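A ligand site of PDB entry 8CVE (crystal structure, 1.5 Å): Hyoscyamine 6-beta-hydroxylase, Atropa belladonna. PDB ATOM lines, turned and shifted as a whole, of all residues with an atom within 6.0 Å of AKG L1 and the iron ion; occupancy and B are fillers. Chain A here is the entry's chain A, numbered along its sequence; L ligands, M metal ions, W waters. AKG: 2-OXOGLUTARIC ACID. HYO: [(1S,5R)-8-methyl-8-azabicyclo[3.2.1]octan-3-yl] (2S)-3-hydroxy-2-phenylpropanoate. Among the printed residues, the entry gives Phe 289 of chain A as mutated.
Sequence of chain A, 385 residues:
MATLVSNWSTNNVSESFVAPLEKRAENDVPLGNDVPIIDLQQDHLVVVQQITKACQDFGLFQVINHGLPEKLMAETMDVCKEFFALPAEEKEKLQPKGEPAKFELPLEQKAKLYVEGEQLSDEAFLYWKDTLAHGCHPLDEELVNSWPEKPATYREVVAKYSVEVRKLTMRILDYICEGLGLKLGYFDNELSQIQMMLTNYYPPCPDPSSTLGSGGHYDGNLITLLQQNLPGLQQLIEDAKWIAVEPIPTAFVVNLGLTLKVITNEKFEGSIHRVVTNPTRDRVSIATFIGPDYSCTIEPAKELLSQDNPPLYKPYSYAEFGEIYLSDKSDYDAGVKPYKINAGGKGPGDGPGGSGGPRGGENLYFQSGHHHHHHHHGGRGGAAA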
ATOM      1  N   LYS A 129      10.419 -17.039 -35.597  1.00  0.00           N
ATOM      2  CA  LYS A 129      11.593 -17.932 -35.698  1.00  0.00           C
ATOM      3  C   LYS A 129      11.755 -18.397 -37.152  1.00  0.00           C
ATOM      4  O   LYS A 129      10.745 -18.732 -37.775  1.00  0.00           O
ATOM      5  CB  LYS A 129      11.390 -19.142 -34.786  1.00  0.00           C
ATOM      6  CG  LYS A 129      12.426 -20.252 -34.886  1.00  0.00           C
ATOM      7  CD  LYS A 129      12.328 -21.252 -33.751  1.00  0.00           C
ATOM      8  CE  LYS A 129      11.138 -22.179 -33.855  1.00  0.00           C
ATOM      9  NZ  LYS A 129      11.308 -23.190 -34.933  1.00  0.00           N
ATOM     10  N   LEU A 198      19.227 -28.222 -35.470  1.00  0.00           N
ATOM     11  CA  LEU A 198      18.309 -27.077 -35.710  1.00  0.00           C
ATOM     12  C   LEU A 198      19.060 -25.800 -35.328  1.00  0.00           C
ATOM     13  O   LEU A 198      19.386 -25.637 -34.135  1.00  0.00           O
ATOM     14  CB  LEU A 198      17.034 -27.259 -34.879  1.00  0.00           C
ATOM     15  CG  LEU A 198      15.955 -28.130 -35.513  1.00  0.00           C
ATOM     16  CD1 LEU A 198      16.426 -29.564 -35.673  1.00  0.00           C
ATOM     17  CD2 LEU A 198      14.679 -28.075 -34.693  1.00  0.00           C
ATOM     18  N   ASN A 200      18.455 -22.027 -34.957  1.00  0.00           N
ATOM     19  CA  ASN A 200      17.264 -21.158 -34.767  1.00  0.00           C
ATOM     20  C   ASN A 200      17.702 -19.698 -34.878  1.00  0.00           C
ATOM     21  O   ASN A 200      18.646 -19.326 -34.185  1.00  0.00           O
ATOM     22  CB  ASN A 200      16.597 -21.408 -33.425  1.00  0.00           C
ATOM     23  CG  ASN A 200      16.193 -22.848 -33.253  1.00  0.00           C
ATOM     24  OD1 ASN A 200      15.471 -23.390 -34.095  1.00  0.00           O
ATOM     25  ND2 ASN A 200      16.650 -23.481 -32.192  1.00  0.00           N
ATOM     26  N   TYR A 202      16.134 -15.919 -34.388  1.00  0.00           N
ATOM     27  CA  TYR A 202      15.079 -15.057 -33.799  1.00  0.00           C
ATOM     28  C   TYR A 202      15.399 -13.611 -34.153  1.00  0.00           C
ATOM     29  O   TYR A 202      16.219 -12.981 -33.481  1.00  0.00           O
ATOM     30  CB  TYR A 202      15.013 -15.277 -32.284  1.00  0.00           C
ATOM     31  CG  TYR A 202      14.898 -16.717 -31.870  1.00  0.00           C
ATOM     32  CD1 TYR A 202      13.661 -17.337 -31.784  1.00  0.00           C
ATOM     33  CD2 TYR A 202      16.021 -17.460 -31.568  1.00  0.00           C
ATOM     34  CE1 TYR A 202      13.551 -18.664 -31.397  1.00  0.00           C
ATOM     35  CE2 TYR A 202      15.925 -18.786 -31.182  1.00  0.00           C
ATOM     36  CZ  TYR A 202      14.686 -19.390 -31.102  1.00  0.00           C
ATOM     37  OH  TYR A 202      14.597 -20.703 -30.717  1.00  0.00           O
ATOM     38  N   SER A 214       9.504 -19.381 -29.609  1.00  0.00           N
ATOM     39  CA  SER A 214       9.194 -20.830 -29.553  1.00  0.00           C
ATOM     40  C   SER A 214       8.164 -21.043 -28.451  1.00  0.00           C
ATOM     41  O   SER A 214       8.442 -20.638 -27.310  1.00  0.00           O
ATOM     42  CB  SER A 214      10.463 -21.618 -29.312  1.00  0.00           C
ATOM     43  OG  SER A 214      10.366 -22.932 -29.849  1.00  0.00           O
ATOM     44  N   HIS A 217       7.173 -26.225 -24.883  1.00  0.00           N
ATOM     45  CA  HIS A 217       7.219 -27.616 -25.400  1.00  0.00           C
ATOM     46  C   HIS A 217       8.229 -28.441 -24.602  1.00  0.00           C
ATOM     47  O   HIS A 217       9.205 -27.869 -24.096  1.00  0.00           O
ATOM     48  CB  HIS A 217       7.586 -27.624 -26.891  1.00  0.00           C
ATOM     49  CG  HIS A 217       8.964 -27.137 -27.193  1.00  0.00           C
ATOM     50  ND1 HIS A 217       9.287 -25.793 -27.185  1.00  0.00           N
ATOM     51  CD2 HIS A 217      10.117 -27.789 -27.488  1.00  0.00           C
ATOM     52  CE1 HIS A 217      10.558 -25.640 -27.474  1.00  0.00           C
ATOM     53  NE2 HIS A 217      11.098 -26.850 -27.664  1.00  0.00           N
ATOM     54  N   TYR A 218       8.017 -29.758 -24.564  1.00  0.00           N
ATOM     55  CA  TYR A 218       9.097 -30.756 -24.456  1.00  0.00           C
ATOM     56  C   TYR A 218       9.734 -30.905 -25.833  1.00  0.00           C
ATOM     57  O   TYR A 218       8.996 -30.840 -26.836  1.00  0.00           O
ATOM     58  CB  TYR A 218       8.588 -32.155 -24.111  1.00  0.00           C
ATOM     59  CG  TYR A 218       7.970 -32.356 -22.752  1.00  0.00           C
ATOM     60  CD1 TYR A 218       8.753 -32.601 -21.629  1.00  0.00           C
ATOM     61  CD2 TYR A 218       6.598 -32.358 -22.594  1.00  0.00           C
ATOM     62  CE1 TYR A 218       8.187 -32.830 -20.390  1.00  0.00           C
ATOM     63  CE2 TYR A 218       6.010 -32.584 -21.360  1.00  0.00           C
ATOM     64  CZ  TYR A 218       6.812 -32.807 -20.250  1.00  0.00           C
ATOM     65  OH  TYR A 218       6.238 -33.040 -19.023  1.00  0.00           O
ATOM     66  N   ASP A 219      11.033 -31.168 -25.884  1.00  0.00           N
ATOM     67  CA  ASP A 219      11.661 -31.798 -27.071  1.00  0.00           C
ATOM     68  C   ASP A 219      11.165 -33.247 -27.099  1.00  0.00           C
ATOM     69  O   ASP A 219      11.257 -33.906 -26.061  1.00  0.00           O
ATOM     70  CB  ASP A 219      13.190 -31.662 -27.022  1.00  0.00           C
ATOM     71  CG  ASP A 219      13.730 -30.237 -27.137  1.00  0.00           C
ATOM     72  OD1 ASP A 219      12.942 -29.299 -27.467  1.00  0.00           O
ATOM     73  OD2 ASP A 219      14.933 -30.077 -26.920  1.00  0.00           O
ATOM     74  N   THR A 224      18.568 -33.350 -26.015  1.00  0.00           N
ATOM     75  CA  THR A 224      18.942 -32.207 -26.886  1.00  0.00           C
ATOM     76  C   THR A 224      20.041 -31.421 -26.182  1.00  0.00           C
ATOM     77  O   THR A 224      19.891 -31.147 -24.982  1.00  0.00           O
ATOM     78  CB  THR A 224      17.735 -31.309 -27.164  1.00  0.00           C
ATOM     79  OG1 THR A 224      16.734 -32.094 -27.820  1.00  0.00           O
ATOM     80  CG2 THR A 224      18.085 -30.123 -28.045  1.00  0.00           C
ATOM     81  N   LEU A 226      21.865 -27.745 -26.400  1.00  0.00           N
ATOM     82  CA  LEU A 226      21.518 -26.399 -26.913  1.00  0.00           C
ATOM     83  C   LEU A 226      22.692 -25.466 -26.621  1.00  0.00           C
ATOM     84  O   LEU A 226      23.142 -25.415 -25.462  1.00  0.00           O
ATOM     85  CB  LEU A 226      20.219 -25.955 -26.238  1.00  0.00           C
ATOM     86  CG  LEU A 226      19.649 -24.591 -26.629  1.00  0.00           C
ATOM     87  CD1 LEU A 226      20.395 -23.442 -25.971  1.00  0.00           C
ATOM     88  CD2 LEU A 226      19.613 -24.406 -28.127  1.00  0.00           C
ATOM     89  N   GLN A 228      23.836 -21.478 -26.767  1.00  0.00           N
ATOM     90  CA  GLN A 228      23.261 -20.118 -26.814  1.00  0.00           C
ATOM     91  C   GLN A 228      24.285 -19.110 -26.294  1.00  0.00           C
ATOM     92  O   GLN A 228      25.092 -19.479 -25.414  1.00  0.00           O
ATOM     93  CB  GLN A 228      21.962 -20.045 -26.004  1.00  0.00           C
ATOM     94  CG  GLN A 228      22.122 -20.477 -24.554  1.00  0.00           C
ATOM     95  CD  GLN A 228      20.960 -20.055 -23.673  1.00  0.00           C
ATOM     96  OE1 GLN A 228      20.013 -19.409 -24.119  1.00  0.00           O
ATOM     97  NE2 GLN A 228      21.039 -20.421 -22.408  1.00  0.00           N
ATOM     98  N   GLY A 232      16.819 -15.490 -23.691  1.00  0.00           N
ATOM     99  CA  GLY A 232      15.542 -15.759 -24.386  1.00  0.00           C
ATOM    100  C   GLY A 232      14.982 -17.117 -24.031  1.00  0.00           C
ATOM    101  O   GLY A 232      13.761 -17.285 -24.147  1.00  0.00           O
ATOM    102  N   LEU A 233      15.836 -18.067 -23.615  1.00  0.00           N
ATOM    103  CA  LEU A 233      15.378 -19.426 -23.242  1.00  0.00           C
ATOM    104  C   LEU A 233      14.787 -19.375 -21.827  1.00  0.00           C
ATOM    105  O   LEU A 233      15.438 -18.833 -20.914  1.00  0.00           O
ATOM    106  CB  LEU A 233      16.547 -20.409 -23.300  1.00  0.00           C
ATOM    107  CG  LEU A 233      16.234 -21.844 -22.872  1.00  0.00           C
ATOM    108  CD1 LEU A 233      15.197 -22.487 -23.787  1.00  0.00           C
ATOM    109  CD2 LEU A 233      17.505 -22.672 -22.822  1.00  0.00           C
ATOM    110  N   ASN A 255      18.703 -30.629 -22.444  1.00  0.00           N
ATOM    111  CA  ASN A 255      17.228 -30.755 -22.313  1.00  0.00           C
ATOM    112  C   ASN A 255      16.872 -32.234 -22.443  1.00  0.00           C
ATOM    113  O   ASN A 255      17.109 -32.788 -23.519  1.00  0.00           O
ATOM    114  CB  ASN A 255      16.489 -29.943 -23.384  1.00  0.00           C
ATOM    115  CG  ASN A 255      16.424 -28.450 -23.123  1.00  0.00           C
ATOM    116  OD1 ASN A 255      16.046 -28.024 -22.034  1.00  0.00           O
ATOM    117  ND2 ASN A 255      16.740 -27.644 -24.119  1.00  0.00           N
ATOM    118  N   HIS A 273      10.174 -25.991 -22.025  1.00  0.00           N
ATOM    119  CA  HIS A 273      10.874 -24.701 -22.248  1.00  0.00           C
ATOM    120  C   HIS A 273      10.228 -23.942 -23.403  1.00  0.00           C
ATOM    121  O   HIS A 273       9.487 -24.541 -24.194  1.00  0.00           O
ATOM    122  CB  HIS A 273      12.375 -24.934 -22.455  1.00  0.00           C
ATOM    123  CG  HIS A 273      12.672 -25.922 -23.535  1.00  0.00           C
ATOM    124  ND1 HIS A 273      12.703 -27.283 -23.314  1.00  0.00           N
ATOM    125  CD2 HIS A 273      12.933 -25.745 -24.850  1.00  0.00           C
ATOM    126  CE1 HIS A 273      12.965 -27.901 -24.455  1.00  0.00           C
ATOM    127  NE2 HIS A 273      13.123 -26.981 -25.403  1.00  0.00           N
ATOM    128  N   ARG A 274      10.502 -22.642 -23.470  1.00  0.00           N
ATOM    129  CA  ARG A 274      10.022 -21.728 -24.535  1.00  0.00           C
ATOM    130  C   ARG A 274      11.130 -20.701 -24.808  1.00  0.00           C
ATOM    131  O   ARG A 274      12.080 -20.618 -24.011  1.00  0.00           O
ATOM    132  CB  ARG A 274       8.716 -21.047 -24.120  1.00  0.00           C
ATOM    133  CG  ARG A 274       8.894 -19.959 -23.075  1.00  0.00           C
ATOM    134  CD  ARG A 274       7.575 -19.400 -22.586  1.00  0.00           C
ATOM    135  NE  ARG A 274       7.818 -18.341 -21.623  1.00  0.00           N
ATOM    136  CZ  ARG A 274       6.888 -17.788 -20.832  1.00  0.00           C
ATOM    137  NH1 ARG A 274       5.629 -18.186 -20.893  1.00  0.00           N
ATOM    138  NH2 ARG A 274       7.231 -16.844 -19.988  1.00  0.00           N
ATOM    139  N   VAL A 275      10.984 -19.948 -25.894  1.00  0.00           N
ATOM    140  CA  VAL A 275      11.908 -18.835 -26.236  1.00  0.00           C
ATOM    141  C   VAL A 275      11.073 -17.570 -26.439  1.00  0.00           C
ATOM    142  O   VAL A 275      10.095 -17.615 -27.206  1.00  0.00           O
ATOM    143  CB  VAL A 275      12.756 -19.158 -27.469  1.00  0.00           C
ATOM    144  CG1 VAL A 275      13.684 -17.992 -27.818  1.00  0.00           C
ATOM    145  CG2 VAL A 275      13.549 -20.442 -27.272  1.00  0.00           C
ATOM    146  N   ARG A 283      19.002 -13.160 -32.339  1.00  0.00           N
ATOM    147  CA  ARG A 283      19.547 -14.257 -31.504  1.00  0.00           C
ATOM    148  C   ARG A 283      19.640 -15.507 -32.371  1.00  0.00           C
ATOM    149  O   ARG A 283      18.673 -15.792 -33.104  1.00  0.00           O
ATOM    150  CB  ARG A 283      18.653 -14.522 -30.294  1.00  0.00           C
ATOM    151  CG  ARG A 283      19.092 -15.690 -29.423  1.00  0.00           C
ATOM    152  CD  ARG A 283      18.284 -15.716 -28.140  1.00  0.00           C
ATOM    153  NE  ARG A 283      18.640 -16.836 -27.284  1.00  0.00           N
ATOM    154  CZ  ARG A 283      18.159 -18.077 -27.387  1.00  0.00           C
ATOM    155  NH1 ARG A 283      17.290 -18.370 -28.340  1.00  0.00           N
ATOM    156  NH2 ARG A 283      18.560 -19.006 -26.546  1.00  0.00           N
ATOM    157  N   SER A 285      20.491 -19.670 -31.854  1.00  0.00           N
ATOM    158  CA  SER A 285      20.766 -20.836 -30.983  1.00  0.00           C
ATOM    159  C   SER A 285      20.998 -22.054 -31.865  1.00  0.00           C
ATOM    160  O   SER A 285      20.466 -22.101 -32.992  1.00  0.00           O
ATOM    161  CB  SER A 285      19.669 -21.063 -29.984  1.00  0.00           C
ATOM    162  OG  SER A 285      18.481 -21.514 -30.609  1.00  0.00           O
ATOM    163  N   ALA A 287      20.701 -26.167 -31.662  1.00  0.00           N
ATOM    164  CA  ALA A 287      20.106 -27.287 -30.908  1.00  0.00           C
ATOM    165  C   ALA A 287      20.408 -28.593 -31.645  1.00  0.00           C
ATOM    166  O   ALA A 287      20.018 -28.706 -32.821  1.00  0.00           O
ATOM    167  CB  ALA A 287      18.623 -27.066 -30.737  1.00  0.00           C
ATOM    168  N   PHE A 289      19.413 -32.305 -31.696  1.00  0.00           N
ATOM    169  CA  PHE A 289      18.295 -33.200 -31.315  1.00  0.00           C
ATOM    170  C   PHE A 289      18.711 -34.648 -31.596  1.00  0.00           C
ATOM    171  O   PHE A 289      18.716 -35.052 -32.762  1.00  0.00           O
ATOM    172  CB  PHE A 289      17.048 -32.851 -32.118  1.00  0.00           C
ATOM    173  CG  PHE A 289      16.275 -31.667 -31.584  1.00  0.00           C
ATOM    174  CD1 PHE A 289      16.756 -30.381 -31.725  1.00  0.00           C
ATOM    175  CD2 PHE A 289      15.068 -31.872 -30.934  1.00  0.00           C
ATOM    176  CE1 PHE A 289      16.022 -29.312 -31.216  1.00  0.00           C
ATOM    177  CE2 PHE A 289      14.341 -30.800 -30.431  1.00  0.00           C
ATOM    178  CZ  PHE A 289      14.837 -29.529 -30.568  1.00  0.00           C
HETATM  179  C1  AKG L   1      14.280 -25.837 -29.795  1.00  0.00           C
HETATM  180  O1  AKG L   1      13.555 -26.805 -29.564  1.00  0.00           O
HETATM  181  O2  AKG L   1      14.729 -25.606 -30.927  1.00  0.00           O
HETATM  182  C2  AKG L   1      14.570 -25.045 -28.796  1.00  0.00           C
HETATM  183  O5  AKG L   1      14.031 -25.274 -27.701  1.00  0.00           O
HETATM  184  C3  AKG L   1      15.535 -23.890 -28.934  1.00  0.00           C
HETATM  185  C4  AKG L   1      15.709 -23.068 -27.675  1.00  0.00           C
HETATM  186  C5  AKG L   1      16.539 -21.798 -27.818  1.00  0.00           C
HETATM  187  O3  AKG L   1      17.215 -21.446 -26.840  1.00  0.00           O
HETATM  188  O4  AKG L   1      16.487 -21.154 -28.888  1.00  0.00           O
HETATM  189  C10 HYO L   2      10.744 -28.687 -34.058  1.00  0.00           C
HETATM  190  C13 HYO L   2      11.471 -31.765 -34.049  1.00  0.00           C
HETATM  191  C15 HYO L   2      11.397 -34.091 -33.332  1.00  0.00           C
HETATM  192  C17 HYO L   2      11.403 -34.781 -32.122  1.00  0.00           C
HETATM  193  C20 HYO L   2       9.792 -35.666 -34.197  1.00  0.00           C
HETATM  194  C21 HYO L   2       9.798 -36.356 -32.987  1.00  0.00           C
HETATM  195  C05 HYO L   2       9.902 -28.527 -31.341  1.00  0.00           C
HETATM  196  C06 HYO L   2      11.298 -27.760 -32.980  1.00  0.00           C
HETATM  197  C07 HYO L   2      11.293 -29.007 -30.916  1.00  0.00           C
HETATM  198  C08 HYO L   2      12.220 -28.514 -32.035  1.00  0.00           C
HETATM  199  C09 HYO L   2       9.176 -29.507 -32.248  1.00  0.00           C
HETATM  200  C11 HYO L   2       9.985 -29.890 -33.482  1.00  0.00           C
HETATM  201  C12 HYO L   2      10.504 -26.180 -31.302  1.00  0.00           C
HETATM  202  C14 HYO L   2      12.280 -32.904 -33.496  1.00  0.00           C
HETATM  203  C16 HYO L   2      13.465 -33.259 -34.388  1.00  0.00           C
HETATM  204  C18 HYO L   2      10.585 -34.546 -34.368  1.00  0.00           C
HETATM  205  C19 HYO L   2      10.604 -35.913 -31.950  1.00  0.00           C
HETATM  206  N04 HYO L   2      10.159 -27.329 -32.148  1.00  0.00           N
HETATM  207  O01 HYO L   2      10.894 -30.906 -33.059  1.00  0.00           O
HETATM  208  O02 HYO L   2      11.287 -31.555 -35.242  1.00  0.00           O
HETATM  209  O03 HYO L   2      14.168 -34.375 -33.813  1.00  0.00           O
HETATM  210 FE    FE M   1      13.224 -27.266 -27.527  1.00  0.00          FE
HETATM  211  O   HOH W   1      13.352 -24.911 -33.286  1.00  0.00           O
HETATM  212  O   HOH W   2      15.590 -27.571 -27.152  1.00  0.00           O
HETATM  213  O   HOH W   3      12.845 -22.968 -30.868  1.00  0.00           O
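The backbone carbonyl oxygen (O) of Ser 214 sits at hydrogen-bond distance from the backbone NH (N) of Val 275, 3.0 Å away.
The guanidinium group (NH2) of Arg 283 sits at hydrogen-bond distance from the side-chain amide oxygen (OE1) of Gln 228 (2.9 Å).
The backbone NH of Tyr 202 lies within hydrogen-bond range of the backbone carbonyl oxygen of Arg 283, at 2.8 Å.
The backbone carbonyl oxygen of Ser 285 lies within hydrogen-bond range of the backbone NH of Asn 200 (2.8 Å).
The side-chain hydroxyl (OG1) of Thr 224 lies within hydrogen-bond range of the side-chain carboxylate (OD2) of Asp 219 (2.8 Å).
Merely in contact with AKG L1: Leu 226 (3.9 Å), Leu 233 (3.7 Å), Val 275 (3.3 Å) and Phe 289 (3.2 Å).
Hydrophobic or aromatic side chains within 4 Å of AKG L1: Tyr 202, His 217, Leu 226, Leu 233, His 273, Val 275 and Phe 289.
Of the 21 residues printed, 11 come within 4 Å of AKG L1.
Along chain A the residues within 4 Å of AKG L1 span positions 200 to 289.
The nearest printed residue that does not touch AKG L1 is Ala 287 (4.2 Å).
The side-chain amide nitrogen (ND2) of Asn 200 is in hydrogen-bond range of an oxygen (O2) of AKG L1.
An oxygen (O4) of AKG L1 is in hydrogen-bond range of the side-chain hydroxyl (OH) of Tyr 202 (2.7 Å).
The guanidinium group (NH2) of Arg 283 lies within salt-bridge range of an oxygen (O3) of AKG L1 (2.8 Å).
The side-chain hydroxyl (OG) of Ser 285 is in hydrogen-bond range of an oxygen (O4) of AKG L1 (2.7 Å).
Water W2 lies within hydrogen-bond range of the side-chain carboxylate of Asp 219 (2.6 Å) and the side-chain amide nitrogen of Asn 255 (3.2 Å).
Water W1 lies within hydrogen-bond range of the side-chain amide oxygen (OD1) of Asn 200 (2.7 Å), an oxygen (O2) of AKG L1 (2.8 Å) and the side-chain amino group (NZ) of Lys 129 (3.1 Å).
Water W3 lies within hydrogen-bond range of OG of Ser 214, OH of Tyr 202 and O2 of AKG L1.
The iron ion is bound by OD1 of Asp 219 (2.1 Å).
The iron ion is bound by O1 of AKG L1, at 2.1 Å.
A ring nitrogen (NE2) of His 273 binds the iron ion, at 2.1 Å.
The iron ion is bound by O5 of AKG L1, at 2.2 Å.
A ring nitrogen (NE2) of His 217 is bound to the iron ion, 2.2 Å away.
The iron ion is bound by water W2, at 2.4 Å.
Of the 21 residues printed, 3 come within 4 Å of the iron ion.
Along chain A the residues within 4 Å of the iron ion span positions 217 to 273.
The nearest printed residue that does not touch the iron ion is Phe 289 (4.1 Å).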
